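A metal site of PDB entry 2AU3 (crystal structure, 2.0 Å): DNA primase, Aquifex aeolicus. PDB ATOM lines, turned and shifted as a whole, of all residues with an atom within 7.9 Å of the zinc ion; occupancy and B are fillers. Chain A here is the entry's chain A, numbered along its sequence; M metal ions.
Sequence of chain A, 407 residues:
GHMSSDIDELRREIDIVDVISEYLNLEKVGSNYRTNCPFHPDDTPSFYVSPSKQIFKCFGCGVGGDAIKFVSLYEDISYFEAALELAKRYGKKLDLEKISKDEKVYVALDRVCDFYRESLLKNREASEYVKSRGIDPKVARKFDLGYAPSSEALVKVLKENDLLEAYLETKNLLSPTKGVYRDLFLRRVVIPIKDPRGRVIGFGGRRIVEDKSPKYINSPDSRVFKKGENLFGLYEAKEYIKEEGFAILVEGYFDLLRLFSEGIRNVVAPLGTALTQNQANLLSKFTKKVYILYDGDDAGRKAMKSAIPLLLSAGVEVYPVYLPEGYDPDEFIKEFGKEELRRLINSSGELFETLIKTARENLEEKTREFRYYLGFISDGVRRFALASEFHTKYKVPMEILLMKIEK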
ATOM      1  N   ASN A  36       0.230  -8.550  24.505  1.00  0.00           N
ATOM      2  CA  ASN A  36      -1.185  -8.243  24.658  1.00  0.00           C
ATOM      3  C   ASN A  36      -1.973  -9.407  24.100  1.00  0.00           C
ATOM      4  O   ASN A  36      -1.599  -9.976  23.079  1.00  0.00           O
ATOM      5  CB  ASN A  36      -1.606  -6.948  23.945  1.00  0.00           C
ATOM      6  CG  ASN A  36      -0.753  -5.757  24.330  1.00  0.00           C
ATOM      7  OD1 ASN A  36      -1.022  -5.062  25.306  1.00  0.00           O
ATOM      8  ND2 ASN A  36       0.274  -5.498  23.531  1.00  0.00           N
ATOM      9  N   CYS A  37      -3.079  -9.737  24.749  1.00  0.00           N
ATOM     10  CA  CYS A  37      -3.890 -10.875  24.319  1.00  0.00           C
ATOM     11  C   CYS A  37      -4.570 -10.624  22.965  1.00  0.00           C
ATOM     12  O   CYS A  37      -5.163  -9.566  22.752  1.00  0.00           O
ATOM     13  CB  CYS A  37      -4.912 -11.222  25.389  1.00  0.00           C
ATOM     14  SG  CYS A  37      -5.867 -12.702  25.028  1.00  0.00           S
ATOM     15  N   PRO A  38      -4.485 -11.585  22.049  1.00  0.00           N
ATOM     16  CA  PRO A  38      -5.138 -11.471  20.736  1.00  0.00           C
ATOM     17  C   PRO A  38      -6.603 -11.922  20.756  1.00  0.00           C
ATOM     18  O   PRO A  38      -7.281 -11.842  19.731  1.00  0.00           O
ATOM     19  CB  PRO A  38      -4.316 -12.428  19.857  1.00  0.00           C
ATOM     20  CG  PRO A  38      -3.879 -13.522  20.827  1.00  0.00           C
ATOM     21  CD  PRO A  38      -3.775 -12.868  22.195  1.00  0.00           C
ATOM     22  N   PHE A  39      -7.068 -12.417  21.906  1.00  0.00           N
ATOM     23  CA  PHE A  39      -8.393 -13.034  21.995  1.00  0.00           C
ATOM     24  C   PHE A  39      -9.412 -12.187  22.791  1.00  0.00           C
ATOM     25  O   PHE A  39     -10.618 -12.313  22.597  1.00  0.00           O
ATOM     26  CB  PHE A  39      -8.303 -14.450  22.575  1.00  0.00           C
ATOM     27  CG  PHE A  39      -7.303 -15.330  21.876  1.00  0.00           C
ATOM     28  CD1 PHE A  39      -7.380 -15.539  20.502  1.00  0.00           C
ATOM     29  CD2 PHE A  39      -6.274 -15.958  22.590  1.00  0.00           C
ATOM     30  CE1 PHE A  39      -6.452 -16.332  19.839  1.00  0.00           C
ATOM     31  CE2 PHE A  39      -5.338 -16.770  21.934  1.00  0.00           C
ATOM     32  CZ  PHE A  39      -5.433 -16.967  20.559  1.00  0.00           C
ATOM     33  N   HIS A  40      -8.902 -11.330  23.671  1.00  0.00           N
ATOM     34  CA  HIS A  40      -9.710 -10.328  24.359  1.00  0.00           C
ATOM     35  C   HIS A  40      -8.978  -8.986  24.344  1.00  0.00           C
ATOM     36  O   HIS A  40      -7.763  -8.946  24.148  1.00  0.00           O
ATOM     37  CB  HIS A  40     -10.035 -10.785  25.794  1.00  0.00           C
ATOM     38  CG  HIS A  40      -9.059 -10.288  26.834  1.00  0.00           C
ATOM     39  ND1 HIS A  40      -7.847 -10.900  27.072  1.00  0.00           N
ATOM     40  CD2 HIS A  40      -9.139  -9.248  27.705  1.00  0.00           C
ATOM     41  CE1 HIS A  40      -7.210 -10.239  28.026  1.00  0.00           C
ATOM     42  NE2 HIS A  40      -7.969  -9.237  28.424  1.00  0.00           N
ATOM     43  N   PRO A  41      -9.693  -7.878  24.495  1.00  0.00           N
ATOM     44  CA  PRO A  41      -9.050  -6.569  24.415  1.00  0.00           C
ATOM     45  C   PRO A  41      -8.742  -5.874  25.738  1.00  0.00           C
ATOM     46  O   PRO A  41      -9.619  -5.157  26.241  1.00  0.00           O
ATOM     47  CB  PRO A  41     -10.090  -5.747  23.644  1.00  0.00           C
ATOM     48  CG  PRO A  41     -11.447  -6.395  23.977  1.00  0.00           C
ATOM     49  CD  PRO A  41     -11.171  -7.762  24.579  1.00  0.00           C
ATOM     50  N   ASP A  42      -7.552  -6.029  26.310  1.00  0.00           N
ATOM     51  CA  ASP A  42      -7.151  -5.023  27.311  1.00  0.00           C
ATOM     52  C   ASP A  42      -5.796  -4.308  27.250  1.00  0.00           C
ATOM     53  O   ASP A  42      -4.764  -4.832  26.816  1.00  0.00           O
ATOM     54  CB  ASP A  42      -7.737  -5.224  28.734  1.00  0.00           C
ATOM     55  CG  ASP A  42      -7.214  -6.459  29.452  1.00  0.00           C
ATOM     56  OD1 ASP A  42      -6.376  -7.198  28.868  1.00  0.00           O
ATOM     57  OD2 ASP A  42      -7.614  -6.748  30.610  1.00  0.00           O
ATOM     58  N   SER A  46      -1.492  -8.987  29.330  1.00  0.00           N
ATOM     59  CA  SER A  46      -1.942  -9.916  30.372  1.00  0.00           C
ATOM     60  C   SER A  46      -1.796 -11.370  29.939  1.00  0.00           C
ATOM     61  O   SER A  46      -2.210 -12.283  30.652  1.00  0.00           O
ATOM     62  CB  SER A  46      -3.414  -9.657  30.705  1.00  0.00           C
ATOM     63  OG  SER A  46      -3.593  -8.298  31.041  1.00  0.00           O
ATOM     64  N   PHE A  47      -1.187 -11.582  28.774  1.00  0.00           N
ATOM     65  CA  PHE A  47      -1.097 -12.886  28.125  1.00  0.00           C
ATOM     66  C   PHE A  47       0.319 -13.409  28.275  1.00  0.00           C
ATOM     67  O   PHE A  47       1.262 -12.833  27.707  1.00  0.00           O
ATOM     68  CB  PHE A  47      -1.475 -12.733  26.649  1.00  0.00           C
ATOM     69  CG  PHE A  47      -1.468 -14.014  25.866  1.00  0.00           C
ATOM     70  CD1 PHE A  47      -2.675 -14.623  25.521  1.00  0.00           C
ATOM     71  CD2 PHE A  47      -0.270 -14.577  25.418  1.00  0.00           C
ATOM     72  CE1 PHE A  47      -2.680 -15.807  24.755  1.00  0.00           C
ATOM     73  CE2 PHE A  47      -0.261 -15.755  24.668  1.00  0.00           C
ATOM     74  CZ  PHE A  47      -1.478 -16.373  24.329  1.00  0.00           C
ATOM     75  N   PHE A  56       0.332 -21.371  27.732  1.00  0.00           N
ATOM     76  CA  PHE A  56       0.078 -19.944  27.768  1.00  0.00           C
ATOM     77  C   PHE A  56      -1.106 -19.773  28.691  1.00  0.00           C
ATOM     78  O   PHE A  56      -1.829 -20.730  28.932  1.00  0.00           O
ATOM     79  CB  PHE A  56      -0.214 -19.386  26.355  1.00  0.00           C
ATOM     80  CG  PHE A  56      -1.529 -19.868  25.761  1.00  0.00           C
ATOM     81  CD1 PHE A  56      -2.709 -19.124  25.926  1.00  0.00           C
ATOM     82  CD2 PHE A  56      -1.592 -21.057  25.022  1.00  0.00           C
ATOM     83  CE1 PHE A  56      -3.927 -19.555  25.364  1.00  0.00           C
ATOM     84  CE2 PHE A  56      -2.831 -21.495  24.468  1.00  0.00           C
ATOM     85  CZ  PHE A  56      -3.986 -20.736  24.644  1.00  0.00           C
ATOM     86  N   LYS A  57      -1.293 -18.576  29.232  1.00  0.00           N
ATOM     87  CA  LYS A  57      -2.463 -18.281  30.066  1.00  0.00           C
ATOM     88  C   LYS A  57      -2.666 -16.778  30.034  1.00  0.00           C
ATOM     89  O   LYS A  57      -1.739 -16.017  30.350  1.00  0.00           O
ATOM     90  CB  LYS A  57      -2.242 -18.743  31.511  1.00  0.00           C
ATOM     91  CG  LYS A  57      -3.421 -18.456  32.473  1.00  0.00           C
ATOM     92  CD  LYS A  57      -4.679 -19.346  32.205  1.00  0.00           C
ATOM     93  CE  LYS A  57      -5.754 -19.083  33.307  1.00  0.00           C
ATOM     94  NZ  LYS A  57      -7.031 -19.847  33.046  1.00  0.00           N
ATOM     95  N   CYS A  58      -3.862 -16.353  29.649  1.00  0.00           N
ATOM     96  CA  CYS A  58      -4.204 -14.944  29.726  1.00  0.00           C
ATOM     97  C   CYS A  58      -4.784 -14.582  31.086  1.00  0.00           C
ATOM     98  O   CYS A  58      -5.815 -15.118  31.481  1.00  0.00           O
ATOM     99  CB  CYS A  58      -5.183 -14.545  28.629  1.00  0.00           C
ATOM    100  SG  CYS A  58      -5.378 -12.772  28.637  1.00  0.00           S
ATOM    101  N   PHE A  59      -4.113 -13.681  31.797  1.00  0.00           N
ATOM    102  CA  PHE A  59      -4.628 -13.204  33.081  1.00  0.00           C
ATOM    103  C   PHE A  59      -5.728 -12.186  32.888  1.00  0.00           C
ATOM    104  O   PHE A  59      -6.287 -11.684  33.850  1.00  0.00           O
ATOM    105  CB  PHE A  59      -3.508 -12.600  33.917  1.00  0.00           C
ATOM    106  CG  PHE A  59      -2.652 -13.619  34.584  1.00  0.00           C
ATOM    107  CD1 PHE A  59      -1.948 -14.557  33.827  1.00  0.00           C
ATOM    108  CD2 PHE A  59      -2.570 -13.665  35.977  1.00  0.00           C
ATOM    109  CE1 PHE A  59      -1.145 -15.520  34.439  1.00  0.00           C
ATOM    110  CE2 PHE A  59      -1.765 -14.625  36.597  1.00  0.00           C
ATOM    111  CZ  PHE A  59      -1.063 -15.557  35.827  1.00  0.00           C
ATOM    112  N   GLY A  60      -6.051 -11.884  31.636  1.00  0.00           N
ATOM    113  CA  GLY A  60      -7.107 -10.933  31.349  1.00  0.00           C
ATOM    114  C   GLY A  60      -8.448 -11.583  31.089  1.00  0.00           C
ATOM    115  O   GLY A  60      -9.465 -11.162  31.641  1.00  0.00           O
ATOM    116  N   CYS A  61      -8.465 -12.607  30.235  1.00  0.00           N
ATOM    117  CA  CYS A  61      -9.687 -13.335  29.967  1.00  0.00           C
ATOM    118  C   CYS A  61      -9.681 -14.784  30.459  1.00  0.00           C
ATOM    119  O   CYS A  61     -10.714 -15.432  30.478  1.00  0.00           O
ATOM    120  CB  CYS A  61     -10.024 -13.302  28.477  1.00  0.00           C
ATOM    121  SG  CYS A  61      -8.815 -14.209  27.481  1.00  0.00           S
ATOM    122  N   GLY A  62      -8.521 -15.307  30.839  1.00  0.00           N
ATOM    123  CA  GLY A  62      -8.431 -16.641  31.406  1.00  0.00           C
ATOM    124  C   GLY A  62      -8.192 -17.761  30.407  1.00  0.00           C
ATOM    125  O   GLY A  62      -7.989 -18.903  30.809  1.00  0.00           O
ATOM    126  N   VAL A  63      -8.221 -17.442  29.120  1.00  0.00           N
ATOM    127  CA  VAL A  63      -7.840 -18.411  28.088  1.00  0.00           C
ATOM    128  C   VAL A  63      -6.425 -18.962  28.373  1.00  0.00           C
ATOM    129  O   VAL A  63      -5.518 -18.229  28.772  1.00  0.00           O
ATOM    130  CB  VAL A  63      -7.957 -17.822  26.652  1.00  0.00           C
ATOM    131  CG1 VAL A  63      -6.742 -17.016  26.254  1.00  0.00           C
ATOM    132  CG2 VAL A  63      -8.207 -18.916  25.652  1.00  0.00           C
ATOM    133  N   GLY A  64      -6.260 -20.261  28.193  1.00  0.00           N
ATOM    134  CA  GLY A  64      -4.985 -20.907  28.463  1.00  0.00           C
ATOM    135  C   GLY A  64      -4.899 -22.235  27.758  1.00  0.00           C
ATOM    136  O   GLY A  64      -5.915 -22.791  27.344  1.00  0.00           O
ATOM    137  N   ARG A 141     -11.024 -16.645  36.787  1.00  0.00           N
ATOM    138  CA  ARG A 141     -10.269 -16.905  35.563  1.00  0.00           C
ATOM    139  C   ARG A 141      -9.161 -17.945  35.707  1.00  0.00           C
ATOM    140  O   ARG A 141      -8.994 -18.803  34.816  1.00  0.00           O
ATOM    141  CB  ARG A 141      -9.679 -15.616  35.036  1.00  0.00           C
ATOM    142  CG  ARG A 141     -10.731 -14.664  34.480  1.00  0.00           C
ATOM    143  CD  ARG A 141     -10.157 -13.444  33.819  1.00  0.00           C
ATOM    144  NE  ARG A 141      -9.385 -12.609  34.744  1.00  0.00           N
ATOM    145  CZ  ARG A 141      -9.816 -11.458  35.287  1.00  0.00           C
ATOM    146  NH1 ARG A 141     -11.045 -10.997  35.028  1.00  0.00           N
ATOM    147  NH2 ARG A 141      -9.019 -10.787  36.096  1.00  0.00           N
HETATM  148 ZN    ZN M   1      -7.087 -12.733  26.949  1.00  0.00          ZN
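The backbone NH of Phe 39 sits close to the side-chain sulfur of Cys 37 (3.4 Å). N of Cys 58 lies within hydrogen-bond range of O of Val 63, 2.7 Å away. The backbone NH (N) of Val 63 lies close to the side-chain sulfur (SG) of Cys 61 (3.7 Å). The backbone NH (N) of Gly 60 lies close to the side-chain sulfur (SG) of Cys 58 (3.2 Å). The backbone carbonyl oxygen of Ser 46 sits close to the side-chain sulfur of Cys 58, 3.8 Å away. A ring nitrogen (NE2) of His 40 sits at hydrogen-bond distance from the side-chain carboxylate of Asp 42 (2.6 Å).
ND1 of His 40 is bound to the zinc ion. SG of Cys 37 is bound to the zinc ion, at 2.3 Å. The side-chain sulfur (SG) of Cys 61 is bound to the zinc ion, 2.3 Å away. SG of Cys 58 is bound to the zinc ion, 2.4 Å away. The zinc ion has four donor atoms within binding distance.
Within 4 Å of the zinc ion: Cys 37, His 40, Cys 58 and Cys 61.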
